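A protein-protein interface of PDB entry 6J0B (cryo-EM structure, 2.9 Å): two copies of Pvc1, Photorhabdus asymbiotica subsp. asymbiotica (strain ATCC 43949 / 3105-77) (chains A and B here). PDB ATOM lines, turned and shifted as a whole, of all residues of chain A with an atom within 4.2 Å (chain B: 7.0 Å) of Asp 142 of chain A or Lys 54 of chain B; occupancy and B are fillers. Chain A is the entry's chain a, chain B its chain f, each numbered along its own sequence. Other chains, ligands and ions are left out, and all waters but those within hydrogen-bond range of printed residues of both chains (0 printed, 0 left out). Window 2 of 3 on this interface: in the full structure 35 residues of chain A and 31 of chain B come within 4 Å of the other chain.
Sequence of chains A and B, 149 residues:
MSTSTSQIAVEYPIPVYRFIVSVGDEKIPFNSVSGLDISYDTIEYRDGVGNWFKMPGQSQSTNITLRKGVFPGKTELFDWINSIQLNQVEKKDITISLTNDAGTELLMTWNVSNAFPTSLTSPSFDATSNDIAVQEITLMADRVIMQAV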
ATOM      1  N   SER A  61      -1.779  13.435   7.217  1.00  0.00           N
ATOM      2  CA  SER A  61      -2.818  12.434   7.408  1.00  0.00           C
ATOM      3  C   SER A  61      -4.175  13.096   7.564  1.00  0.00           C
ATOM      4  O   SER A  61      -4.307  14.136   8.213  1.00  0.00           O
ATOM      5  CB  SER A  61      -2.519  11.571   8.632  1.00  0.00           C
ATOM      6  OG  SER A  61      -3.278  10.375   8.600  1.00  0.00           O
ATOM      7  N   LYS A  91     -11.031  -1.444   8.029  1.00  0.00           N
ATOM      8  CA  LYS A  91     -11.077  -0.134   7.405  1.00  0.00           C
ATOM      9  C   LYS A  91     -12.071  -0.167   6.258  1.00  0.00           C
ATOM     10  O   LYS A  91     -12.196  -1.176   5.561  1.00  0.00           O
ATOM     11  CB  LYS A  91      -9.699   0.267   6.892  1.00  0.00           C
ATOM     12  CG  LYS A  91      -8.597   0.086   7.899  1.00  0.00           C
ATOM     13  CD  LYS A  91      -7.289   0.578   7.344  1.00  0.00           C
ATOM     14  CE  LYS A  91      -6.259   0.720   8.429  1.00  0.00           C
ATOM     15  NZ  LYS A  91      -5.000   1.288   7.892  1.00  0.00           N
ATOM     16  N   SER A 113     -10.551   7.036   1.700  1.00  0.00           N
ATOM     17  CA  SER A 113     -10.061   5.671   1.622  1.00  0.00           C
ATOM     18  C   SER A 113      -9.495   5.239   2.964  1.00  0.00           C
ATOM     19  O   SER A 113      -8.857   6.038   3.654  1.00  0.00           O
ATOM     20  CB  SER A 113      -8.982   5.540   0.551  1.00  0.00           C
ATOM     21  OG  SER A 113      -9.481   5.908  -0.719  1.00  0.00           O
ATOM     22  N   ASN A 114      -9.750   3.975   3.322  1.00  0.00           N
ATOM     23  CA  ASN A 114      -9.116   3.286   4.452  1.00  0.00           C
ATOM     24  C   ASN A 114      -9.371   3.984   5.784  1.00  0.00           C
ATOM     25  O   ASN A 114      -8.474   4.098   6.618  1.00  0.00           O
ATOM     26  CB  ASN A 114      -7.611   3.118   4.232  1.00  0.00           C
ATOM     27  CG  ASN A 114      -7.279   2.128   3.145  1.00  0.00           C
ATOM     28  OD1 ASN A 114      -6.464   2.397   2.268  1.00  0.00           O
ATOM     29  ND2 ASN A 114      -7.887   0.967   3.212  1.00  0.00           N
ATOM     30  N   PHE A 116     -10.644   4.387   9.511  1.00  0.00           N
ATOM     31  CA  PHE A 116     -10.843   3.543  10.674  1.00  0.00           C
ATOM     32  C   PHE A 116     -11.073   4.427  11.890  1.00  0.00           C
ATOM     33  O   PHE A 116     -10.579   5.554  11.931  1.00  0.00           O
ATOM     34  CB  PHE A 116      -9.642   2.599  10.887  1.00  0.00           C
ATOM     35  CG  PHE A 116      -8.349   3.288  11.214  1.00  0.00           C
ATOM     36  CD1 PHE A 116      -7.517   3.726  10.207  1.00  0.00           C
ATOM     37  CD2 PHE A 116      -7.939   3.442  12.528  1.00  0.00           C
ATOM     38  CE1 PHE A 116      -6.335   4.341  10.500  1.00  0.00           C
ATOM     39  CE2 PHE A 116      -6.756   4.062  12.821  1.00  0.00           C
ATOM     40  CZ  PHE A 116      -5.952   4.508  11.808  1.00  0.00           C
ATOM     41  N   MET A 140      -9.433   8.444  11.129  1.00  0.00           N
ATOM     42  CA  MET A 140      -8.163   8.710  10.479  1.00  0.00           C
ATOM     43  C   MET A 140      -8.136   7.963   9.159  1.00  0.00           C
ATOM     44  O   MET A 140      -8.524   6.796   9.093  1.00  0.00           O
ATOM     45  CB  MET A 140      -6.983   8.288  11.352  1.00  0.00           C
ATOM     46  CG  MET A 140      -5.637   8.544  10.700  1.00  0.00           C
ATOM     47  SD  MET A 140      -4.232   8.271  11.772  1.00  0.00           S
ATOM     48  CE  MET A 140      -4.274   9.783  12.715  1.00  0.00           C
ATOM     49  N   ALA A 141      -7.694   8.638   8.106  1.00  0.00           N
ATOM     50  CA  ALA A 141      -7.728   8.041   6.784  1.00  0.00           C
ATOM     51  C   ALA A 141      -6.658   8.670   5.909  1.00  0.00           C
ATOM     52  O   ALA A 141      -5.809   9.435   6.371  1.00  0.00           O
ATOM     53  CB  ALA A 141      -9.103   8.208   6.155  1.00  0.00           C
ATOM     54  N   ASP A 142      -6.718   8.333   4.627  1.00  0.00           N
ATOM     55  CA  ASP A 142      -5.846   8.872   3.602  1.00  0.00           C
ATOM     56  C   ASP A 142      -6.665   9.092   2.341  1.00  0.00           C
ATOM     57  O   ASP A 142      -7.714   8.472   2.155  1.00  0.00           O
ATOM     58  CB  ASP A 142      -4.694   7.921   3.305  1.00  0.00           C
ATOM     59  CG  ASP A 142      -5.150   6.485   3.230  1.00  0.00           C
ATOM     60  OD1 ASP A 142      -5.985   6.098   4.068  1.00  0.00           O
ATOM     61  OD2 ASP A 142      -4.689   5.746   2.339  1.00  0.00           O
ATOM     62  N   ARG A 143      -6.165   9.984   1.482  1.00  0.00           N
ATOM     63  CA  ARG A 143      -6.677  10.211   0.128  1.00  0.00           C
ATOM     64  C   ARG A 143      -8.150  10.641   0.137  1.00  0.00           C
ATOM     65  O   ARG A 143      -9.073   9.856  -0.088  1.00  0.00           O
ATOM     66  CB  ARG A 143      -6.457   9.000  -0.784  1.00  0.00           C
ATOM     67  CG  ARG A 143      -6.822   9.308  -2.228  1.00  0.00           C
ATOM     68  CD  ARG A 143      -5.769   8.921  -3.181  1.00  0.00           C
ATOM     69  NE  ARG A 143      -6.047   9.353  -4.546  1.00  0.00           N
ATOM     70  CZ  ARG A 143      -6.868   8.735  -5.389  1.00  0.00           C
ATOM     71  NH1 ARG A 143      -7.033   9.221  -6.610  1.00  0.00           N
ATOM     72  NH2 ARG A 143      -7.535   7.649  -5.021  1.00  0.00           N
ATOM     73  N   VAL A 144      -8.353  11.889   0.525  1.00  0.00           N
ATOM     74  CA  VAL A 144      -9.573  12.583   0.134  1.00  0.00           C
ATOM     75  C   VAL A 144      -9.440  12.989  -1.322  1.00  0.00           C
ATOM     76  O   VAL A 144      -8.488  13.680  -1.697  1.00  0.00           O
ATOM     77  CB  VAL A 144      -9.826  13.806   1.015  1.00  0.00           C
ATOM     78  CG1 VAL A 144     -11.078  14.523   0.567  1.00  0.00           C
ATOM     79  CG2 VAL A 144      -9.978  13.357   2.380  1.00  0.00           C
ATOM     80  N   THR B  42      -2.882   6.621  17.411  1.00  0.00           N
ATOM     81  CA  THR B  42      -2.684   6.078  16.077  1.00  0.00           C
ATOM     82  C   THR B  42      -1.201   5.869  15.833  1.00  0.00           C
ATOM     83  O   THR B  42      -0.389   6.752  16.117  1.00  0.00           O
ATOM     84  CB  THR B  42      -3.266   6.995  15.005  1.00  0.00           C
ATOM     85  OG1 THR B  42      -2.423   8.142  14.848  1.00  0.00           O
ATOM     86  CG2 THR B  42      -4.657   7.442  15.401  1.00  0.00           C
ATOM     87  N   ILE B  43      -0.857   4.702  15.312  1.00  0.00           N
ATOM     88  CA  ILE B  43       0.513   4.360  14.972  1.00  0.00           C
ATOM     89  C   ILE B  43       0.667   4.481  13.467  1.00  0.00           C
ATOM     90  O   ILE B  43      -0.141   3.934  12.709  1.00  0.00           O
ATOM     91  CB  ILE B  43       0.863   2.944  15.447  1.00  0.00           C
ATOM     92  CG1 ILE B  43       0.320   2.690  16.844  1.00  0.00           C
ATOM     93  CG2 ILE B  43       2.319   2.799  15.530  1.00  0.00           C
ATOM     94  CD1 ILE B  43       0.599   1.294  17.341  1.00  0.00           C
ATOM     95  N   GLU B  44       1.698   5.195  13.026  1.00  0.00           N
ATOM     96  CA  GLU B  44       1.918   5.451  11.609  1.00  0.00           C
ATOM     97  C   GLU B  44       3.307   4.977  11.210  1.00  0.00           C
ATOM     98  O   GLU B  44       4.308   5.485  11.722  1.00  0.00           O
ATOM     99  CB  GLU B  44       1.740   6.935  11.290  1.00  0.00           C
ATOM    100  CG  GLU B  44       0.335   7.446  11.556  1.00  0.00           C
ATOM    101  CD  GLU B  44       0.169   8.914  11.228  1.00  0.00           C
ATOM    102  OE1 GLU B  44       1.186   9.634  11.180  1.00  0.00           O
ATOM    103  OE2 GLU B  44      -0.983   9.345  11.016  1.00  0.00           O
ATOM    104  N   TYR B  45       3.362   4.002  10.304  1.00  0.00           N
ATOM    105  CA  TYR B  45       4.599   3.566   9.669  1.00  0.00           C
ATOM    106  C   TYR B  45       4.634   4.113   8.260  1.00  0.00           C
ATOM    107  O   TYR B  45       3.606   4.157   7.583  1.00  0.00           O
ATOM    108  CB  TYR B  45       4.718   2.050   9.590  1.00  0.00           C
ATOM    109  CG  TYR B  45       6.051   1.550   9.097  1.00  0.00           C
ATOM    110  CD1 TYR B  45       7.218   1.772   9.814  1.00  0.00           C
ATOM    111  CD2 TYR B  45       6.133   0.837   7.918  1.00  0.00           C
ATOM    112  CE1 TYR B  45       8.428   1.302   9.353  1.00  0.00           C
ATOM    113  CE2 TYR B  45       7.326   0.367   7.453  1.00  0.00           C
ATOM    114  CZ  TYR B  45       8.470   0.600   8.168  1.00  0.00           C
ATOM    115  OH  TYR B  45       9.656   0.117   7.679  1.00  0.00           O
ATOM    116  N   TRP B  52       2.059   3.950   3.209  1.00  0.00           N
ATOM    117  CA  TRP B  52       1.879   4.598   4.498  1.00  0.00           C
ATOM    118  C   TRP B  52       0.855   3.795   5.281  1.00  0.00           C
ATOM    119  O   TRP B  52      -0.315   3.736   4.894  1.00  0.00           O
ATOM    120  CB  TRP B  52       1.410   6.036   4.293  1.00  0.00           C
ATOM    121  CG  TRP B  52       1.418   6.903   5.490  1.00  0.00           C
ATOM    122  CD1 TRP B  52       1.906   6.608   6.719  1.00  0.00           C
ATOM    123  CD2 TRP B  52       0.912   8.233   5.568  1.00  0.00           C
ATOM    124  NE1 TRP B  52       1.733   7.670   7.566  1.00  0.00           N
ATOM    125  CE2 TRP B  52       1.123   8.684   6.879  1.00  0.00           C
ATOM    126  CE3 TRP B  52       0.296   9.088   4.651  1.00  0.00           C
ATOM    127  CZ2 TRP B  52       0.743   9.949   7.300  1.00  0.00           C
ATOM    128  CZ3 TRP B  52      -0.083  10.339   5.070  1.00  0.00           C
ATOM    129  CH2 TRP B  52       0.145  10.759   6.381  1.00  0.00           C
ATOM    130  N   PHE B  53       1.293   3.170   6.365  1.00  0.00           N
ATOM    131  CA  PHE B  53       0.427   2.335   7.183  1.00  0.00           C
ATOM    132  C   PHE B  53      -0.090   3.144   8.360  1.00  0.00           C
ATOM    133  O   PHE B  53       0.696   3.734   9.100  1.00  0.00           O
ATOM    134  CB  PHE B  53       1.171   1.105   7.694  1.00  0.00           C
ATOM    135  CG  PHE B  53       1.764   0.260   6.612  1.00  0.00           C
ATOM    136  CD1 PHE B  53       3.110   0.330   6.329  1.00  0.00           C
ATOM    137  CD2 PHE B  53       0.977  -0.608   5.883  1.00  0.00           C
ATOM    138  CE1 PHE B  53       3.664  -0.447   5.342  1.00  0.00           C
ATOM    139  CE2 PHE B  53       1.524  -1.387   4.892  1.00  0.00           C
ATOM    140  CZ  PHE B  53       2.869  -1.307   4.623  1.00  0.00           C
ATOM    141  N   LYS B  54      -1.405   3.169   8.529  1.00  0.00           N
ATOM    142  CA  LYS B  54      -2.037   3.756   9.699  1.00  0.00           C
ATOM    143  C   LYS B  54      -2.744   2.656  10.474  1.00  0.00           C
ATOM    144  O   LYS B  54      -3.455   1.836   9.888  1.00  0.00           O
ATOM    145  CB  LYS B  54      -3.024   4.853   9.310  1.00  0.00           C
ATOM    146  CG  LYS B  54      -2.423   6.236   9.250  1.00  0.00           C
ATOM    147  CD  LYS B  54      -1.867   6.539   7.886  1.00  0.00           C
ATOM    148  CE  LYS B  54      -2.973   6.720   6.876  1.00  0.00           C
ATOM    149  NZ  LYS B  54      -2.420   6.842   5.505  1.00  0.00           N
ATOM    150  N   MET B  55      -2.539   2.636  11.783  1.00  0.00           N
ATOM    151  CA  MET B  55      -3.053   1.590  12.646  1.00  0.00           C
ATOM    152  C   MET B  55      -3.703   2.204  13.871  1.00  0.00           C
ATOM    153  O   MET B  55      -3.314   3.288  14.306  1.00  0.00           O
ATOM    154  CB  MET B  55      -1.932   0.651  13.102  1.00  0.00           C
ATOM    155  CG  MET B  55      -1.504  -0.363  12.086  1.00  0.00           C
ATOM    156  SD  MET B  55       0.102  -1.044  12.496  1.00  0.00           S
ATOM    157  CE  MET B  55       1.136   0.354  12.095  1.00  0.00           C
ATOM    158  N   PRO B  56      -4.699   1.539  14.444  1.00  0.00           N
ATOM    159  CA  PRO B  56      -5.122   1.901  15.794  1.00  0.00           C
ATOM    160  C   PRO B  56      -4.083   1.427  16.787  1.00  0.00           C
ATOM    161  O   PRO B  56      -3.513   0.345  16.645  1.00  0.00           O
ATOM    162  CB  PRO B  56      -6.445   1.154  15.974  1.00  0.00           C
ATOM    163  CG  PRO B  56      -6.820   0.688  14.638  1.00  0.00           C
ATOM    164  CD  PRO B  56      -5.569   0.507  13.867  1.00  0.00           C
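NZ of Lys 91 of chain A sits at hydrogen-bond distance from O of Lys 54 of chain B (2.6 Å).
SD of Met 140 of chain A sits close to OG1 of Thr 42 of chain B, 3.6 Å away.
OE2 of Glu 44 of chain B is in hydrogen-bond range of OG of Ser 61 of chain A.
OD1 of Asp 142 of chain A is in salt-bridge range of NZ of Lys 54 of chain B.
The side-chain sulfur (SD) of Met 140 of chain A lies close to the side-chain carboxylate (OE2) of Glu 44 of chain B, at 3.5 Å.
The backbone NH (N) of Met 140 of chain A is in hydrogen-bond range of the backbone carbonyl oxygen (O) of Phe 116 of chain A (3.2 Å).
The backbone NH of Ser 113 of chain A lies within hydrogen-bond range of the backbone carbonyl oxygen of Asp 142 of chain A.
O of Ile 43 of chain B sits at hydrogen-bond distance from N of Met 55 of chain B.
Among the printed residues, pairs that only touch across the chains: Ser 61 of chain A with Trp 52 of chain B, Phe 116 of chain A with Lys 54 of chain B, Phe 116 of chain A with Pro 56 of chain B, Met 140 of chain A with Lys 54 of chain B, Phe 116 of chain A with Met 55 of chain B and Ala 141 of chain A with Lys 54 of chain B.
Asp 142 of chain A touches just one residue of chain B: Lys 54 (3.3 Å).
Of chain A, only Lys 91, Phe 116, Met 140, Ala 141 and Asp 142 come within 4 Å of Lys 54 of chain B.
Of the printed residues of chain B, Met 140 of chain A touches Thr 42 (3.3 Å), Glu 44 (3.5 Å) and Lys 54 (3.7 Å).
Printed residues of chain A within 4 Å of Met 55 of chain B: Phe 116 (3.7 Å).
Of the printed residues of chain A, Thr 42 of chain B touches Met 140 (3.3 Å).
Printed residues of chain B within 4 Å of Phe 116 of chain A: Lys 54, Met 55 and Pro 56.
Asn 114 of chain A touches none of the printed residues of chain B.
Printed residues of chain A that touch a printed residue of chain B: Ser 61, Lys 91, Phe 116, Met 140, Ala 141 and Asp 142.
Hydrophobic or aromatic side chains of chain A within 4 Å of the printed part of chain B: Phe 116 and Met 140.
Along chain A the printed residues that touch a printed residue of chain B span positions 61 to 142.
Of the 9 printed residues of chain B, 6 touch a printed residue of chain A.
Printed residues of chain B that touch a printed residue of chain A: Thr 42, Glu 44, Trp 52, Lys 54, Met 55 and Pro 56.
Hydrophobic or aromatic side chains of chain B within 4 Å of the printed part of chain A: Trp 52 and Pro 56.
Among the printed residues, 11 pairs touch across the chains.
Among the printed residues, Asp or Glu carboxylates within 4 Å of a Lys or Arg side-chain nitrogen of the other chain: Asp 142 of chain A with Lys 54 of chain B (3.9 Å).
No position is printed for both chains.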
